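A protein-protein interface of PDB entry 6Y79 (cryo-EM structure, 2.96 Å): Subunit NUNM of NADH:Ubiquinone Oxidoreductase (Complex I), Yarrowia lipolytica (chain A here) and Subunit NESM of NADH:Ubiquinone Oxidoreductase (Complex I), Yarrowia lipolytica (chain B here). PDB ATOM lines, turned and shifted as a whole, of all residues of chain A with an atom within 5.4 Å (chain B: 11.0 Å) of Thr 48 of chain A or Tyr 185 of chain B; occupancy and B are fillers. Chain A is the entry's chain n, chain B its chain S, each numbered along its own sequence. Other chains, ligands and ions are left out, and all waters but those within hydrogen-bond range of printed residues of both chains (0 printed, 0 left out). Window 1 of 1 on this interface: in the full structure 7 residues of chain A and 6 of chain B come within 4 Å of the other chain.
The side-chain hydroxyl of Tyr 185 of chain B is in hydrogen-bond range of the side-chain amide nitrogen of Asn 38 of chain A (2.8 Å).
NH1 of Arg 188 of chain B lies within hydrogen-bond range of OH of Tyr 35 of chain A (3.3 Å).
The side-chain amide nitrogen (ND2) of Asn 38 of chain A lies within hydrogen-bond range of the backbone carbonyl oxygen (O) of Phe 34 of chain A.
OD1 of Asn 38 of chain A is in hydrogen-bond range of N of Trp 49 of chain A (3.3 Å).
The backbone NH (N) of Thr 48 of chain A is in hydrogen-bond range of the side-chain carboxylate (OE1) of Glu 42 of chain A, 3.0 Å away.
OG1 of Thr 48 of chain A sits at hydrogen-bond distance from OE1 of Glu 51 of chain A (3.1 Å).
Among the printed residues, merely in contact across the chains: Phe 34 of chain A with Tyr 185 of chain B (3.7 Å), Tyr 35 of chain A with Tyr 185 of chain B (3.3 Å), Thr 48 of chain A with Tyr 185 of chain B (3.6 Å), Phe 54 of chain A with Tyr 185 of chain B (3.6 Å), Phe 54 of chain A with Lys 186 of chain B (3.96 Å) and Phe 54 of chain A with Glu 189 of chain B (3.2 Å).
Of chain B, only Tyr 185 (3.6 Å) comes within 4 Å of Thr 48 of chain A.
Of chain A, only Phe 34, Tyr 35, Asn 38, Thr 48 and Phe 54 come within 4 Å of Tyr 185 of chain B.
Asn 38 of chain A touches one residue of chain B.
No residue of chain B comes within 4 Å of Tyr 41 of chain A.
No residue of chain B comes within 4 Å of Glu 42 of chain A.
No residue of chain B comes within 4 Å of Gly 46 of chain A.
No residue of chain B comes within 4 Å of His 47 of chain A.
No residue of chain B comes within 4 Å of Val 50 of chain A.
No residue of chain B comes within 4 Å of Glu 51 of chain A.
Of the printed residues of chain B, Phe 34 of chain A touches Tyr 185.
Of the printed residues of chain A, Glu 189 of chain B touches Phe 54 (3.2 Å).
Of the printed residues of chain A, Arg 188 of chain B touches Tyr 35.
Hydrophobic or aromatic side chains of chain A that line the printed part of chain B: Phe 34, Tyr 35 and Phe 54.
Of the 15 printed residues of chain B, 4 touch a printed residue of chain A.
Along chain B the printed residues that touch a printed residue of chain A span positions 185 to 189.
Among the printed residues, 8 pairs touch across the chains.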
ATOM      1  N   PHE A  34      20.390 -14.435  32.659  1.00  0.00           N
ATOM      2  CA  PHE A  34      19.412 -14.804  31.645  1.00  0.00           C
ATOM      3  C   PHE A  34      18.539 -15.967  32.102  1.00  0.00           C
ATOM      4  O   PHE A  34      17.335 -16.005  31.803  1.00  0.00           O
ATOM      5  CB  PHE A  34      20.127 -15.147  30.344  1.00  0.00           C
ATOM      6  CG  PHE A  34      19.201 -15.365  29.196  1.00  0.00           C
ATOM      7  CD1 PHE A  34      18.450 -14.314  28.695  1.00  0.00           C
ATOM      8  CD2 PHE A  34      19.071 -16.616  28.618  1.00  0.00           C
ATOM      9  CE1 PHE A  34      17.590 -14.506  27.644  1.00  0.00           C
ATOM     10  CE2 PHE A  34      18.212 -16.814  27.564  1.00  0.00           C
ATOM     11  CZ  PHE A  34      17.471 -15.756  27.078  1.00  0.00           C
ATOM     12  N   TYR A  35      19.129 -16.921  32.834  1.00  0.00           N
ATOM     13  CA  TYR A  35      18.348 -18.015  33.402  1.00  0.00           C
ATOM     14  C   TYR A  35      17.328 -17.500  34.411  1.00  0.00           C
ATOM     15  O   TYR A  35      16.163 -17.930  34.413  1.00  0.00           O
ATOM     16  CB  TYR A  35      19.280 -19.036  34.051  1.00  0.00           C
ATOM     17  CG  TYR A  35      18.561 -20.252  34.569  1.00  0.00           C
ATOM     18  CD1 TYR A  35      18.202 -21.279  33.714  1.00  0.00           C
ATOM     19  CD2 TYR A  35      18.230 -20.366  35.912  1.00  0.00           C
ATOM     20  CE1 TYR A  35      17.536 -22.387  34.181  1.00  0.00           C
ATOM     21  CE2 TYR A  35      17.560 -21.464  36.385  1.00  0.00           C
ATOM     22  CZ  TYR A  35      17.218 -22.472  35.518  1.00  0.00           C
ATOM     23  OH  TYR A  35      16.548 -23.568  35.995  1.00  0.00           O
ATOM     24  N   ASN A  38      14.434 -15.862  32.531  1.00  0.00           N
ATOM     25  CA  ASN A  38      13.431 -16.797  32.024  1.00  0.00           C
ATOM     26  C   ASN A  38      12.574 -17.364  33.145  1.00  0.00           C
ATOM     27  O   ASN A  38      11.371 -17.570  32.960  1.00  0.00           O
ATOM     28  CB  ASN A  38      14.096 -17.916  31.236  1.00  0.00           C
ATOM     29  CG  ASN A  38      14.642 -17.438  29.926  1.00  0.00           C
ATOM     30  OD1 ASN A  38      13.921 -17.343  28.942  1.00  0.00           O
ATOM     31  ND2 ASN A  38      15.916 -17.109  29.907  1.00  0.00           N
ATOM     32  N   TYR A  41      10.080 -14.706  33.762  1.00  0.00           N
ATOM     33  CA  TYR A  41       9.101 -14.559  32.689  1.00  0.00           C
ATOM     34  C   TYR A  41       8.115 -15.724  32.645  1.00  0.00           C
ATOM     35  O   TYR A  41       6.956 -15.547  32.224  1.00  0.00           O
ATOM     36  CB  TYR A  41       9.889 -14.415  31.394  1.00  0.00           C
ATOM     37  CG  TYR A  41       9.118 -14.118  30.158  1.00  0.00           C
ATOM     38  CD1 TYR A  41       8.804 -12.814  29.815  1.00  0.00           C
ATOM     39  CD2 TYR A  41       8.766 -15.134  29.291  1.00  0.00           C
ATOM     40  CE1 TYR A  41       8.129 -12.535  28.657  1.00  0.00           C
ATOM     41  CE2 TYR A  41       8.091 -14.869  28.131  1.00  0.00           C
ATOM     42  CZ  TYR A  41       7.777 -13.569  27.819  1.00  0.00           C
ATOM     43  OH  TYR A  41       7.098 -13.305  26.659  1.00  0.00           O
ATOM     44  N   GLU A  42       8.563 -16.906  33.086  1.00  0.00           N
ATOM     45  CA  GLU A  42       7.716 -18.089  33.108  1.00  0.00           C
ATOM     46  C   GLU A  42       6.528 -17.904  34.052  1.00  0.00           C
ATOM     47  O   GLU A  42       5.405 -18.303  33.732  1.00  0.00           O
ATOM     48  CB  GLU A  42       8.560 -19.283  33.535  1.00  0.00           C
ATOM     49  CG  GLU A  42       7.795 -20.557  33.757  1.00  0.00           C
ATOM     50  CD  GLU A  42       7.462 -21.263  32.477  1.00  0.00           C
ATOM     51  OE1 GLU A  42       8.271 -21.159  31.540  1.00  0.00           O
ATOM     52  OE2 GLU A  42       6.393 -21.894  32.419  1.00  0.00           O
ATOM     53  N   GLY A  46       3.478 -18.067  31.680  1.00  0.00           N
ATOM     54  CA  GLY A  46       3.250 -19.484  31.518  1.00  0.00           C
ATOM     55  C   GLY A  46       4.230 -20.199  30.618  1.00  0.00           C
ATOM     56  O   GLY A  46       4.132 -21.425  30.478  1.00  0.00           O
ATOM     57  N   HIS A  47       5.173 -19.485  30.011  1.00  0.00           N
ATOM     58  CA  HIS A  47       6.144 -20.118  29.133  1.00  0.00           C
ATOM     59  C   HIS A  47       7.429 -19.298  29.118  1.00  0.00           C
ATOM     60  O   HIS A  47       7.423 -18.098  29.402  1.00  0.00           O
ATOM     61  CB  HIS A  47       5.588 -20.278  27.712  1.00  0.00           C
ATOM     62  CG  HIS A  47       5.308 -18.980  27.023  1.00  0.00           C
ATOM     63  ND1 HIS A  47       4.206 -18.204  27.312  1.00  0.00           N
ATOM     64  CD2 HIS A  47       5.988 -18.320  26.057  1.00  0.00           C
ATOM     65  CE1 HIS A  47       4.217 -17.124  26.553  1.00  0.00           C
ATOM     66  NE2 HIS A  47       5.289 -17.170  25.782  1.00  0.00           N
ATOM     67  N   THR A  48       8.523 -19.974  28.772  1.00  0.00           N
ATOM     68  CA  THR A  48       9.875 -19.431  28.681  1.00  0.00           C
ATOM     69  C   THR A  48       9.944 -18.362  27.576  1.00  0.00           C
ATOM     70  O   THR A  48       9.138 -18.348  26.643  1.00  0.00           O
ATOM     71  CB  THR A  48      10.843 -20.603  28.436  1.00  0.00           C
ATOM     72  OG1 THR A  48      10.623 -21.596  29.447  1.00  0.00           O
ATOM     73  CG2 THR A  48      12.326 -20.221  28.480  1.00  0.00           C
ATOM     74  N   TRP A  49      10.904 -17.435  27.700  1.00  0.00           N
ATOM     75  CA  TRP A  49      11.132 -16.450  26.648  1.00  0.00           C
ATOM     76  C   TRP A  49      11.838 -17.077  25.445  1.00  0.00           C
ATOM     77  O   TRP A  49      11.722 -16.588  24.321  1.00  0.00           O
ATOM     78  CB  TRP A  49      11.945 -15.269  27.180  1.00  0.00           C
ATOM     79  CG  TRP A  49      12.088 -14.214  26.134  1.00  0.00           C
ATOM     80  CD1 TRP A  49      11.100 -13.421  25.641  1.00  0.00           C
ATOM     81  CD2 TRP A  49      13.268 -13.891  25.389  1.00  0.00           C
ATOM     82  NE1 TRP A  49      11.593 -12.602  24.660  1.00  0.00           N
ATOM     83  CE2 TRP A  49      12.923 -12.870  24.486  1.00  0.00           C
ATOM     84  CE3 TRP A  49      14.584 -14.356  25.411  1.00  0.00           C
ATOM     85  CZ2 TRP A  49      13.844 -12.305  23.613  1.00  0.00           C
ATOM     86  CZ3 TRP A  49      15.499 -13.794  24.543  1.00  0.00           C
ATOM     87  CH2 TRP A  49      15.125 -12.778  23.656  1.00  0.00           C
ATOM     88  N   VAL A  50      12.595 -18.154  25.649  1.00  0.00           N
ATOM     89  CA  VAL A  50      13.310 -18.737  24.517  1.00  0.00           C
ATOM     90  C   VAL A  50      12.405 -19.673  23.724  1.00  0.00           C
ATOM     91  O   VAL A  50      12.542 -19.761  22.502  1.00  0.00           O
ATOM     92  CB  VAL A  50      14.606 -19.395  25.030  1.00  0.00           C
ATOM     93  CG1 VAL A  50      15.305 -20.239  23.972  1.00  0.00           C
ATOM     94  CG2 VAL A  50      15.547 -18.320  25.462  1.00  0.00           C
ATOM     95  N   GLU A  51      11.399 -20.293  24.352  1.00  0.00           N
ATOM     96  CA  GLU A  51      10.481 -21.131  23.580  1.00  0.00           C
ATOM     97  C   GLU A  51       9.494 -20.304  22.749  1.00  0.00           C
ATOM     98  O   GLU A  51       8.704 -20.878  21.993  1.00  0.00           O
ATOM     99  CB  GLU A  51       9.753 -22.111  24.499  1.00  0.00           C
ATOM    100  CG  GLU A  51       8.687 -21.518  25.393  1.00  0.00           C
ATOM    101  CD  GLU A  51       8.118 -22.532  26.372  1.00  0.00           C
ATOM    102  OE1 GLU A  51       8.862 -22.984  27.263  1.00  0.00           O
ATOM    103  OE2 GLU A  51       6.930 -22.888  26.248  1.00  0.00           O
ATOM    104  N   THR A  52       9.511 -18.966  22.881  1.00  0.00           N
ATOM    105  CA  THR A  52       8.939 -18.104  21.848  1.00  0.00           C
ATOM    106  C   THR A  52       9.573 -18.371  20.490  1.00  0.00           C
ATOM    107  O   THR A  52       8.882 -18.354  19.467  1.00  0.00           O
ATOM    108  CB  THR A  52       9.146 -16.626  22.182  1.00  0.00           C
ATOM    109  OG1 THR A  52      10.556 -16.343  22.223  1.00  0.00           O
ATOM    110  CG2 THR A  52       8.512 -16.253  23.505  1.00  0.00           C
ATOM    111  N   PHE A  54      11.164 -21.151  19.534  1.00  0.00           N
ATOM    112  CA  PHE A  54      11.124 -22.553  19.135  1.00  0.00           C
ATOM    113  C   PHE A  54       9.917 -22.726  18.237  1.00  0.00           C
ATOM    114  O   PHE A  54       8.777 -22.753  18.708  1.00  0.00           O
ATOM    115  CB  PHE A  54      11.026 -23.482  20.341  1.00  0.00           C
ATOM    116  CG  PHE A  54      12.260 -23.534  21.194  1.00  0.00           C
ATOM    117  CD1 PHE A  54      13.459 -22.979  20.775  1.00  0.00           C
ATOM    118  CD2 PHE A  54      12.213 -24.163  22.422  1.00  0.00           C
ATOM    119  CE1 PHE A  54      14.574 -23.037  21.574  1.00  0.00           C
ATOM    120  CE2 PHE A  54      13.323 -24.225  23.223  1.00  0.00           C
ATOM    121  CZ  PHE A  54      14.505 -23.661  22.798  1.00  0.00           C
ATOM    122  N   ILE B 177      27.803 -20.365  22.587  1.00  0.00           N
ATOM    123  CA  ILE B 177      26.953 -20.028  23.728  1.00  0.00           C
ATOM    124  C   ILE B 177      25.480 -20.112  23.341  1.00  0.00           C
ATOM    125  O   ILE B 177      24.639 -20.536  24.147  1.00  0.00           O
ATOM    126  CB  ILE B 177      27.345 -18.636  24.264  1.00  0.00           C
ATOM    127  CG1 ILE B 177      28.740 -18.681  24.862  1.00  0.00           C
ATOM    128  CG2 ILE B 177      26.379 -18.123  25.319  1.00  0.00           C
ATOM    129  CD1 ILE B 177      29.354 -17.330  25.033  1.00  0.00           C
ATOM    130  N   LEU B 178      25.152 -19.761  22.096  1.00  0.00           N
ATOM    131  CA  LEU B 178      23.805 -19.951  21.580  1.00  0.00           C
ATOM    132  C   LEU B 178      23.427 -21.425  21.591  1.00  0.00           C
ATOM    133  O   LEU B 178      22.344 -21.761  22.055  1.00  0.00           O
ATOM    134  CB  LEU B 178      23.704 -19.365  20.161  1.00  0.00           C
ATOM    135  CG  LEU B 178      22.344 -18.910  19.586  1.00  0.00           C
ATOM    136  CD1 LEU B 178      22.549 -17.788  18.588  1.00  0.00           C
ATOM    137  CD2 LEU B 178      21.556 -20.041  18.904  1.00  0.00           C
ATOM    138  N   LEU B 179      24.330 -22.302  21.141  1.00  0.00           N
ATOM    139  CA  LEU B 179      24.121 -23.749  21.170  1.00  0.00           C
ATOM    140  C   LEU B 179      23.858 -24.251  22.581  1.00  0.00           C
ATOM    141  O   LEU B 179      22.968 -25.083  22.782  1.00  0.00           O
ATOM    142  CB  LEU B 179      25.340 -24.460  20.573  1.00  0.00           C
ATOM    143  CG  LEU B 179      25.325 -25.957  20.217  1.00  0.00           C
ATOM    144  CD1 LEU B 179      26.116 -26.186  18.966  1.00  0.00           C
ATOM    145  CD2 LEU B 179      25.944 -26.767  21.304  1.00  0.00           C
ATOM    146  N   LEU B 180      24.610 -23.735  23.561  1.00  0.00           N
ATOM    147  CA  LEU B 180      24.374 -24.068  24.969  1.00  0.00           C
ATOM    148  C   LEU B 180      22.973 -23.673  25.416  1.00  0.00           C
ATOM    149  O   LEU B 180      22.274 -24.459  26.062  1.00  0.00           O
ATOM    150  CB  LEU B 180      25.409 -23.370  25.852  1.00  0.00           C
ATOM    151  CG  LEU B 180      25.487 -23.651  27.361  1.00  0.00           C
ATOM    152  CD1 LEU B 180      26.899 -23.489  27.768  1.00  0.00           C
ATOM    153  CD2 LEU B 180      24.654 -22.722  28.242  1.00  0.00           C
ATOM    154  N   ILE B 181      22.568 -22.439  25.111  1.00  0.00           N
ATOM    155  CA  ILE B 181      21.269 -21.935  25.556  1.00  0.00           C
ATOM    156  C   ILE B 181      20.130 -22.691  24.875  1.00  0.00           C
ATOM    157  O   ILE B 181      19.112 -23.013  25.515  1.00  0.00           O
ATOM    158  CB  ILE B 181      21.200 -20.415  25.308  1.00  0.00           C
ATOM    159  CG1 ILE B 181      22.166 -19.688  26.241  1.00  0.00           C
ATOM    160  CG2 ILE B 181      19.815 -19.869  25.527  1.00  0.00           C
ATOM    161  CD1 ILE B 181      22.499 -18.295  25.789  1.00  0.00           C
ATOM    162  N   VAL B 182      20.309 -23.046  23.597  1.00  0.00           N
ATOM    163  CA  VAL B 182      19.265 -23.791  22.905  1.00  0.00           C
ATOM    164  C   VAL B 182      19.181 -25.205  23.469  1.00  0.00           C
ATOM    165  O   VAL B 182      18.084 -25.731  23.638  1.00  0.00           O
ATOM    166  CB  VAL B 182      19.474 -23.785  21.377  1.00  0.00           C
ATOM    167  CG1 VAL B 182      18.404 -24.604  20.658  1.00  0.00           C
ATOM    168  CG2 VAL B 182      19.421 -22.362  20.865  1.00  0.00           C
ATOM    169  N   MET B 183      20.307 -25.806  23.872  1.00  0.00           N
ATOM    170  CA  MET B 183      20.254 -27.135  24.487  1.00  0.00           C
ATOM    171  C   MET B 183      19.621 -27.099  25.869  1.00  0.00           C
ATOM    172  O   MET B 183      18.887 -28.021  26.239  1.00  0.00           O
ATOM    173  CB  MET B 183      21.649 -27.729  24.593  1.00  0.00           C
ATOM    174  CG  MET B 183      22.201 -28.226  23.309  1.00  0.00           C
ATOM    175  SD  MET B 183      23.883 -28.790  23.511  1.00  0.00           S
ATOM    176  CE  MET B 183      23.567 -30.448  24.058  1.00  0.00           C
ATOM    177  N   VAL B 184      19.915 -26.060  26.652  1.00  0.00           N
ATOM    178  CA  VAL B 184      19.413 -25.983  28.019  1.00  0.00           C
ATOM    179  C   VAL B 184      17.908 -25.758  28.028  1.00  0.00           C
ATOM    180  O   VAL B 184      17.170 -26.444  28.747  1.00  0.00           O
ATOM    181  CB  VAL B 184      20.162 -24.885  28.798  1.00  0.00           C
ATOM    182  CG1 VAL B 184      19.418 -24.503  30.065  1.00  0.00           C
ATOM    183  CG2 VAL B 184      21.552 -25.358  29.150  1.00  0.00           C
ATOM    184  N   TYR B 185      17.417 -24.828  27.210  1.00  0.00           N
ATOM    185  CA  TYR B 185      15.980 -24.609  27.186  1.00  0.00           C
ATOM    186  C   TYR B 185      15.239 -25.582  26.291  1.00  0.00           C
ATOM    187  O   TYR B 185      14.014 -25.680  26.403  1.00  0.00           O
ATOM    188  CB  TYR B 185      15.658 -23.182  26.766  1.00  0.00           C
ATOM    189  CG  TYR B 185      16.089 -22.188  27.795  1.00  0.00           C
ATOM    190  CD1 TYR B 185      15.420 -22.079  29.000  1.00  0.00           C
ATOM    191  CD2 TYR B 185      17.179 -21.374  27.570  1.00  0.00           C
ATOM    192  CE1 TYR B 185      15.823 -21.175  29.946  1.00  0.00           C
ATOM    193  CE2 TYR B 185      17.588 -20.471  28.507  1.00  0.00           C
ATOM    194  CZ  TYR B 185      16.907 -20.375  29.688  1.00  0.00           C
ATOM    195  OH  TYR B 185      17.323 -19.467  30.619  1.00  0.00           O
ATOM    196  N   LYS B 186      15.935 -26.306  25.416  1.00  0.00           N
ATOM    197  CA  LYS B 186      15.286 -27.371  24.672  1.00  0.00           C
ATOM    198  C   LYS B 186      15.118 -28.614  25.535  1.00  0.00           C
ATOM    199  O   LYS B 186      14.322 -29.495  25.200  1.00  0.00           O
ATOM    200  CB  LYS B 186      16.091 -27.652  23.393  1.00  0.00           C
ATOM    201  CG  LYS B 186      15.438 -28.580  22.370  1.00  0.00           C
ATOM    202  CD  LYS B 186      14.295 -27.931  21.622  1.00  0.00           C
ATOM    203  CE  LYS B 186      14.789 -27.098  20.468  1.00  0.00           C
ATOM    204  NZ  LYS B 186      13.695 -26.813  19.506  1.00  0.00           N
ATOM    205  N   SER B 187      15.821 -28.686  26.663  1.00  0.00           N
ATOM    206  CA  SER B 187      15.709 -29.830  27.558  1.00  0.00           C
ATOM    207  C   SER B 187      14.453 -29.787  28.414  1.00  0.00           C
ATOM    208  O   SER B 187      14.144 -30.784  29.073  1.00  0.00           O
ATOM    209  CB  SER B 187      16.935 -29.918  28.458  1.00  0.00           C
ATOM    210  OG  SER B 187      16.824 -31.005  29.358  1.00  0.00           O
ATOM    211  N   ARG B 188      13.753 -28.651  28.456  1.00  0.00           N
ATOM    212  CA  ARG B 188      12.430 -28.584  29.066  1.00  0.00           C
ATOM    213  C   ARG B 188      11.479 -29.538  28.359  1.00  0.00           C
ATOM    214  O   ARG B 188      10.715 -30.277  28.988  1.00  0.00           O
ATOM    215  CB  ARG B 188      11.897 -27.152  28.991  1.00  0.00           C
ATOM    216  CG  ARG B 188      12.827 -26.103  29.549  1.00  0.00           C
ATOM    217  CD  ARG B 188      12.764 -26.100  31.050  1.00  0.00           C
ATOM    218  NE  ARG B 188      13.668 -25.127  31.645  1.00  0.00           N
ATOM    219  CZ  ARG B 188      13.696 -24.845  32.942  1.00  0.00           C
ATOM    220  NH1 ARG B 188      14.548 -23.946  33.410  1.00  0.00           N
ATOM    221  NH2 ARG B 188      12.868 -25.466  33.774  1.00  0.00           N
ATOM    222  N   GLU B 189      11.541 -29.526  27.033  1.00  0.00           N
ATOM    223  CA  GLU B 189      10.743 -30.367  26.145  1.00  0.00           C
ATOM    224  C   GLU B 189      11.327 -31.765  26.157  1.00  0.00           C
ATOM    225  O   GLU B 189      12.132 -32.120  25.297  1.00  0.00           O
ATOM    226  CB  GLU B 189      10.767 -29.810  24.727  1.00  0.00           C
ATOM    227  CG  GLU B 189      10.137 -28.442  24.480  1.00  0.00           C
ATOM    228  CD  GLU B 189      11.048 -27.280  24.890  1.00  0.00           C
ATOM    229  OE1 GLU B 189      12.092 -27.536  25.520  1.00  0.00           O
ATOM    230  OE2 GLU B 189      10.749 -26.131  24.537  1.00  0.00           O
ATOM    231  N   ASP B 190      10.954 -32.578  27.141  1.00  0.00           N
ATOM    232  CA  ASP B 190      11.324 -33.979  27.068  1.00  0.00           C
ATOM    233  C   ASP B 190      10.225 -34.878  27.610  1.00  0.00           C
ATOM    234  O   ASP B 190       9.214 -34.420  28.149  1.00  0.00           O
ATOM    235  CB  ASP B 190      12.704 -34.271  27.745  1.00  0.00           C
ATOM    236  CG  ASP B 190      12.742 -34.090  29.273  1.00  0.00           C
ATOM    237  OD1 ASP B 190      11.816 -34.442  30.042  1.00  0.00           O
ATOM    238  OD2 ASP B 190      13.796 -33.601  29.719  1.00  0.00           O
ATOM    239  N   PHE B 193       9.093 -35.078  31.812  1.00  0.00           N
ATOM    240  CA  PHE B 193       8.141 -34.069  32.275  1.00  0.00           C
ATOM    241  C   PHE B 193       6.773 -34.279  31.637  1.00  0.00           C
ATOM    242  O   PHE B 193       5.738 -34.253  32.321  1.00  0.00           O
ATOM    243  CB  PHE B 193       8.650 -32.660  31.954  1.00  0.00           C
ATOM    244  CG  PHE B 193       9.870 -32.245  32.733  1.00  0.00           C
ATOM    245  CD1 PHE B 193       9.768 -31.821  34.047  1.00  0.00           C
ATOM    246  CD2 PHE B 193      11.112 -32.234  32.126  1.00  0.00           C
ATOM    247  CE1 PHE B 193      10.899 -31.427  34.751  1.00  0.00           C
ATOM    248  CE2 PHE B 193      12.239 -31.845  32.820  1.00  0.00           C
ATOM    249  CZ  PHE B 193      12.131 -31.441  34.128  1.00  0.00           C
